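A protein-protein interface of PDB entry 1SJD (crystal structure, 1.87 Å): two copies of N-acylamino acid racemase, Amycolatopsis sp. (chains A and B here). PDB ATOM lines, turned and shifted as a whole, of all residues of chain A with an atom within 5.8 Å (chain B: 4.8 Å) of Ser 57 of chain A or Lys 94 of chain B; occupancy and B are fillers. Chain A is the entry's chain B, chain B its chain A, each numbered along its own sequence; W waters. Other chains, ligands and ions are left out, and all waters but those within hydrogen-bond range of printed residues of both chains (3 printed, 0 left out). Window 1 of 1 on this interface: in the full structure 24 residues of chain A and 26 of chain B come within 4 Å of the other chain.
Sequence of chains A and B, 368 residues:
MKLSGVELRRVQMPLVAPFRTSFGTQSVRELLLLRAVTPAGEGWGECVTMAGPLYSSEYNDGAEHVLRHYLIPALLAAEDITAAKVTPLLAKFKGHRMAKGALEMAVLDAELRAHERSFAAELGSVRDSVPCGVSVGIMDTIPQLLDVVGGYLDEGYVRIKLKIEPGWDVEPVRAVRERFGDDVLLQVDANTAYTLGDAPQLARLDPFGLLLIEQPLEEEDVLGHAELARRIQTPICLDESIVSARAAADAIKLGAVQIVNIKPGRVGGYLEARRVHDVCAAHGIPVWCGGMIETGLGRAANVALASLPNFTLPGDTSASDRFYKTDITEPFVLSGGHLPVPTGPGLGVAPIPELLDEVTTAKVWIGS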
ATOM      1  N   PRO A  53      15.776  14.495 -17.538  1.00  0.00           N
ATOM      2  CA  PRO A  53      15.002  13.304 -17.883  1.00  0.00           C
ATOM      3  C   PRO A  53      13.607  13.329 -17.320  1.00  0.00           C
ATOM      4  O   PRO A  53      13.299  12.574 -16.399  1.00  0.00           O
ATOM      5  CB  PRO A  53      15.733  12.156 -17.201  1.00  0.00           C
ATOM      6  CG  PRO A  53      16.508  12.788 -16.051  1.00  0.00           C
ATOM      7  CD  PRO A  53      16.715  14.254 -16.422  1.00  0.00           C
ATOM      8  N   LEU A  54      12.763  14.175 -17.877  1.00  0.00           N
ATOM      9  CA  LEU A  54      11.396  14.301 -17.382  1.00  0.00           C
ATOM     10  C   LEU A  54      10.330  13.636 -18.202  1.00  0.00           C
ATOM     11  O   LEU A  54       9.305  13.299 -17.606  1.00  0.00           O
ATOM     12  CB  LEU A  54      11.018  15.769 -17.225  1.00  0.00           C
ATOM     13  CG  LEU A  54      11.956  16.487 -16.272  1.00  0.00           C
ATOM     14  CD1 LEU A  54      11.417  17.874 -16.010  1.00  0.00           C
ATOM     15  CD2 LEU A  54      12.189  15.712 -14.966  1.00  0.00           C
ATOM     16  N   TYR A  55      10.544  13.553 -19.542  1.00  0.00           N
ATOM     17  CA  TYR A  55       9.581  12.894 -20.443  1.00  0.00           C
ATOM     18  C   TYR A  55       9.979  11.442 -20.576  1.00  0.00           C
ATOM     19  O   TYR A  55       9.113  10.572 -20.733  1.00  0.00           O
ATOM     20  CB  TYR A  55       9.377  13.559 -21.832  1.00  0.00           C
ATOM     21  CG  TYR A  55       8.890  12.643 -22.968  1.00  0.00           C
ATOM     22  CD1 TYR A  55       9.825  11.874 -23.669  1.00  0.00           C
ATOM     23  CD2 TYR A  55       7.552  12.626 -23.404  1.00  0.00           C
ATOM     24  CE1 TYR A  55       9.401  11.057 -24.718  1.00  0.00           C
ATOM     25  CE2 TYR A  55       7.110  11.826 -24.463  1.00  0.00           C
ATOM     26  CZ  TYR A  55       8.064  11.028 -25.114  1.00  0.00           C
ATOM     27  OH  TYR A  55       7.738  10.199 -26.173  1.00  0.00           O
ATOM     28  N   SER A  56      11.315  11.218 -20.467  1.00  0.00           N
ATOM     29  CA  SER A  56      11.947   9.909 -20.531  1.00  0.00           C
ATOM     30  C   SER A  56      13.299   9.981 -19.854  1.00  0.00           C
ATOM     31  O   SER A  56      13.667  11.061 -19.402  1.00  0.00           O
ATOM     32  CB  SER A  56      12.068   9.363 -21.948  1.00  0.00           C
ATOM     33  OG  SER A  56      13.164   9.976 -22.597  1.00  0.00           O
ATOM     34  N   SER A  57      13.998   8.833 -19.763  1.00  0.00           N
ATOM     35  CA  SER A  57      15.290   8.754 -19.089  1.00  0.00           C
ATOM     36  C   SER A  57      16.395   9.533 -19.760  1.00  0.00           C
ATOM     37  O   SER A  57      17.389   9.885 -19.127  1.00  0.00           O
ATOM     38  CB  SER A  57      15.755   7.330 -18.834  1.00  0.00           C
ATOM     39  OG  SER A  57      16.012   6.669 -20.058  1.00  0.00           O
ATOM     40  N   GLU A  58      16.240   9.777 -21.055  1.00  0.00           N
ATOM     41  CA  GLU A  58      17.256  10.524 -21.798  1.00  0.00           C
ATOM     42  C   GLU A  58      17.240  12.041 -21.607  1.00  0.00           C
ATOM     43  O   GLU A  58      16.209  12.676 -21.476  1.00  0.00           O
ATOM     44  CB  GLU A  58      17.315  10.146 -23.295  1.00  0.00           C
ATOM     45  CG  GLU A  58      17.542   8.635 -23.534  1.00  0.00           C
ATOM     46  CD  GLU A  58      17.498   8.378 -24.994  1.00  0.00           C
ATOM     47  OE1 GLU A  58      16.544   7.900 -25.559  1.00  0.00           O
ATOM     48  OE2 GLU A  58      18.579   8.760 -25.595  1.00  0.00           O
ATOM     49  N   TYR A  59      18.424  12.630 -21.604  1.00  0.00           N
ATOM     50  CA  TYR A  59      18.526  14.061 -21.471  1.00  0.00           C
ATOM     51  C   TYR A  59      19.803  14.589 -22.153  1.00  0.00           C
ATOM     52  O   TYR A  59      20.798  13.865 -22.399  1.00  0.00           O
ATOM     53  CB  TYR A  59      18.286  14.575 -20.047  1.00  0.00           C
ATOM     54  CG  TYR A  59      19.395  14.131 -19.145  1.00  0.00           C
ATOM     55  CD1 TYR A  59      19.377  12.824 -18.654  1.00  0.00           C
ATOM     56  CD2 TYR A  59      20.450  14.980 -18.783  1.00  0.00           C
ATOM     57  CE1 TYR A  59      20.368  12.369 -17.780  1.00  0.00           C
ATOM     58  CE2 TYR A  59      21.464  14.518 -17.934  1.00  0.00           C
ATOM     59  CZ  TYR A  59      21.422  13.219 -17.417  1.00  0.00           C
ATOM     60  OH  TYR A  59      22.415  12.772 -16.537  1.00  0.00           O
ATOM     61  N   ASN A 191       0.693  12.603 -20.703  1.00  0.00           N
ATOM     62  CA  ASN A 191       2.130  12.414 -20.504  1.00  0.00           C
ATOM     63  C   ASN A 191       2.397  11.619 -19.247  1.00  0.00           C
ATOM     64  O   ASN A 191       3.261  12.041 -18.463  1.00  0.00           O
ATOM     65  CB  ASN A 191       2.996  13.704 -20.465  1.00  0.00           C
ATOM     66  CG  ASN A 191       3.191  14.343 -21.838  1.00  0.00           C
ATOM     67  OD1 ASN A 191       2.815  15.497 -22.062  1.00  0.00           O
ATOM     68  ND2 ASN A 191       3.796  13.609 -22.781  1.00  0.00           N
ATOM     69  N   THR A 192       1.636  10.500 -19.102  1.00  0.00           N
ATOM     70  CA  THR A 192       1.738   9.489 -18.028  1.00  0.00           C
ATOM     71  C   THR A 192       1.170   9.922 -16.694  1.00  0.00           C
ATOM     72  O   THR A 192       1.363   9.223 -15.705  1.00  0.00           O
ATOM     73  CB  THR A 192       3.218   8.980 -17.833  1.00  0.00           C
ATOM     74  OG1 THR A 192       3.984   9.915 -17.106  1.00  0.00           O
ATOM     75  CG2 THR A 192       3.976   8.832 -19.159  1.00  0.00           C
ATOM     76  N   GLU A 218       1.759   5.234 -17.135  1.00  0.00           N
ATOM     77  CA  GLU A 218       3.188   5.237 -17.265  1.00  0.00           C
ATOM     78  C   GLU A 218       3.704   4.458 -18.458  1.00  0.00           C
ATOM     79  O   GLU A 218       3.087   3.539 -18.961  1.00  0.00           O
ATOM     80  CB  GLU A 218       3.865   4.776 -15.983  1.00  0.00           C
ATOM     81  CG  GLU A 218       3.455   3.362 -15.558  1.00  0.00           C
ATOM     82  CD  GLU A 218       4.185   2.916 -14.319  1.00  0.00           C
ATOM     83  OE1 GLU A 218       4.788   3.681 -13.586  1.00  0.00           O
ATOM     84  OE2 GLU A 218       4.082   1.617 -14.134  1.00  0.00           O
ATOM     85  N   GLU A 219       4.882   4.818 -18.899  1.00  0.00           N
ATOM     86  CA  GLU A 219       5.457   4.214 -20.064  1.00  0.00           C
ATOM     87  C   GLU A 219       5.503   2.703 -20.078  1.00  0.00           C
ATOM     88  O   GLU A 219       5.315   2.051 -21.124  1.00  0.00           O
ATOM     89  CB  GLU A 219       6.870   4.763 -20.265  1.00  0.00           C
ATOM     90  CG  GLU A 219       7.593   3.934 -21.333  1.00  0.00           C
ATOM     91  CD  GLU A 219       9.028   4.334 -21.418  1.00  0.00           C
ATOM     92  OE1 GLU A 219       9.476   5.352 -20.930  1.00  0.00           O
ATOM     93  OE2 GLU A 219       9.743   3.456 -22.037  1.00  0.00           O
ATOM     94  N   ALA B  91      10.698  10.341  -8.128  1.00  0.00           N
ATOM     95  CA  ALA B  91       9.801   9.897  -9.163  1.00  0.00           C
ATOM     96  C   ALA B  91       9.763  10.744 -10.440  1.00  0.00           C
ATOM     97  O   ALA B  91       9.569  10.249 -11.547  1.00  0.00           O
ATOM     98  CB  ALA B  91       8.425   9.736  -8.563  1.00  0.00           C
ATOM     99  N   LYS B  92       9.904  12.044 -10.304  1.00  0.00           N
ATOM    100  CA  LYS B  92       9.883  12.924 -11.459  1.00  0.00           C
ATOM    101  C   LYS B  92      10.968  12.587 -12.478  1.00  0.00           C
ATOM    102  O   LYS B  92      10.851  12.915 -13.660  1.00  0.00           O
ATOM    103  CB  LYS B  92       9.957  14.386 -11.045  1.00  0.00           C
ATOM    104  CG  LYS B  92      11.276  14.780 -10.400  1.00  0.00           C
ATOM    105  CD  LYS B  92      11.247  16.171  -9.782  1.00  0.00           C
ATOM    106  CE  LYS B  92      11.314  17.263 -10.834  1.00  0.00           C
ATOM    107  NZ  LYS B  92      11.448  18.607 -10.262  1.00  0.00           N
ATOM    108  N   PHE B  93      12.026  11.923 -12.029  1.00  0.00           N
ATOM    109  CA  PHE B  93      13.103  11.530 -12.922  1.00  0.00           C
ATOM    110  C   PHE B  93      12.851  10.150 -13.461  1.00  0.00           C
ATOM    111  O   PHE B  93      12.753   9.193 -12.696  1.00  0.00           O
ATOM    112  CB  PHE B  93      14.456  11.586 -12.227  1.00  0.00           C
ATOM    113  CG  PHE B  93      14.622  12.935 -11.592  1.00  0.00           C
ATOM    114  CD1 PHE B  93      14.762  13.044 -10.210  1.00  0.00           C
ATOM    115  CD2 PHE B  93      14.628  14.102 -12.365  1.00  0.00           C
ATOM    116  CE1 PHE B  93      14.938  14.294  -9.613  1.00  0.00           C
ATOM    117  CE2 PHE B  93      14.797  15.363 -11.784  1.00  0.00           C
ATOM    118  CZ  PHE B  93      14.948  15.451 -10.400  1.00  0.00           C
ATOM    119  N   LYS B  94      12.707  10.081 -14.776  1.00  0.00           N
ATOM    120  CA  LYS B  94      12.410   8.838 -15.480  1.00  0.00           C
ATOM    121  C   LYS B  94      13.625   7.927 -15.577  1.00  0.00           C
ATOM    122  O   LYS B  94      14.712   8.393 -15.920  1.00  0.00           O
ATOM    123  CB  LYS B  94      11.922   9.175 -16.885  1.00  0.00           C
ATOM    124  CG  LYS B  94      10.795  10.195 -16.851  1.00  0.00           C
ATOM    125  CD  LYS B  94       9.479   9.544 -16.417  1.00  0.00           C
ATOM    126  CE  LYS B  94       8.247  10.105 -17.127  1.00  0.00           C
ATOM    127  NZ  LYS B  94       6.958   9.614 -16.613  1.00  0.00           N
ATOM    128  N   GLY B  95      13.414   6.634 -15.263  1.00  0.00           N
ATOM    129  CA  GLY B  95      14.443   5.600 -15.336  1.00  0.00           C
ATOM    130  C   GLY B  95      15.516   5.738 -14.284  1.00  0.00           C
ATOM    131  O   GLY B  95      15.210   6.077 -13.148  1.00  0.00           O
ATOM    132  N   HIS B  96      16.761   5.427 -14.671  1.00  0.00           N
ATOM    133  CA  HIS B  96      17.928   5.521 -13.792  1.00  0.00           C
ATOM    134  C   HIS B  96      17.816   4.749 -12.505  1.00  0.00           C
ATOM    135  O   HIS B  96      18.265   5.238 -11.468  1.00  0.00           O
ATOM    136  CB  HIS B  96      18.171   6.976 -13.429  1.00  0.00           C
ATOM    137  CG  HIS B  96      18.496   7.727 -14.684  1.00  0.00           C
ATOM    138  ND1 HIS B  96      19.763   7.656 -15.257  1.00  0.00           N
ATOM    139  CD2 HIS B  96      17.704   8.516 -15.483  1.00  0.00           C
ATOM    140  CE1 HIS B  96      19.729   8.404 -16.360  1.00  0.00           C
ATOM    141  NE2 HIS B  96      18.516   8.938 -16.521  1.00  0.00           N
HETATM  142  O   HOH W   1       8.775  13.699 -14.949  1.00  0.00           O
HETATM  143  O   HOH W   2       6.221  12.419 -17.761  1.00  0.00           O
HETATM  144  O   HOH W   3       6.772   6.670 -17.747  1.00  0.00           O
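O of Pro 53 of chain A sits at hydrogen-bond distance from N of Lys 94 of chain B (3.0 Å).
OG1 of Thr 192 of chain A sits at hydrogen-bond distance from NZ of Lys 94 of chain B.
The backbone carbonyl oxygen (O) of Ser 57 of chain A lies within hydrogen-bond range of a ring nitrogen (NE2) of His 96 of chain B (3.0 Å).
The side-chain hydroxyl (OG) of Ser 56 of chain A sits close to the backbone NH (N) of Glu 58 of chain A.
Among the printed residues, merely in contact across the chains: Pro 53 of chain A with Lys 92 of chain B (3.7 Å), Pro 53 of chain A with Phe 93 of chain B (3.6 Å), Leu 54 of chain A with Lys 92 of chain B (3.4 Å), Leu 54 of chain A with Phe 93 of chain B (3.9 Å), Leu 54 of chain A with Lys 94 of chain B (3.4 Å), Tyr 55 of chain A with Lys 94 of chain B (3.7 Å), Ser 56 of chain A with Lys 94 of chain B (3.4 Å) and Ser 57 of chain A with Lys 94 of chain B (3.2 Å).
Of chain B, only Lys 94 (3.2 Å) and His 96 (3.0 Å) come within 4 Å of Ser 57 of chain A.
Of chain A, only Pro 53, Leu 54, Tyr 55, Ser 56, Ser 57 and Thr 192 come within 4 Å of Lys 94 of chain B.
Printed residues of chain B within 4 Å of Ser 56 of chain A: Lys 94.
Of the printed residues of chain B, Thr 192 of chain A touches Lys 94.
Printed residues of chain A within 4 Å of Phe 93 of chain B: Pro 53 (3.6 Å) and Leu 54 (3.9 Å).
Of the printed residues of chain B, Pro 53 of chain A touches Lys 92 (3.7 Å), Phe 93 (3.6 Å) and Lys 94 (3.0 Å).
The nearest residue of chain A that does not touch Lys 94 of chain B is Asn 191 of chain A (4.8 Å).
The nearest printed residue of chain B that does not touch Thr 192 of chain A is Ala 91 of chain B (7.9 Å).
Of the 11 printed residues of chain A, 6 touch a printed residue of chain B.
Hydrophobic or aromatic side chains of chain A that line the printed part of chain B: Leu 54.
Of the 6 printed residues of chain B, 4 touch a printed residue of chain A.
No position is printed for both chains.
Of the 11 pairs that touch across the chains among the printed residues, none has its exchanged pair printed and touching as well.
Water W1 bridges O of Lys 92 of chain B (2.6 Å) and O of Leu 54 of chain A (2.7 Å).
Water W3 bridges the backbone NH of Glu 219 of chain A (2.9 Å) and the side-chain amino group of Lys 94 of chain B (3.2 Å).
Water W2 lies within hydrogen-bond range of the backbone carbonyl oxygen (O) of Asn 191 of chain A, the side-chain amino group (NZ) of Lys 94 of chain B, the backbone carbonyl oxygen (O) of Leu 54 of chain A and the side-chain hydroxyl (OG1) of Thr 192 of chain A.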
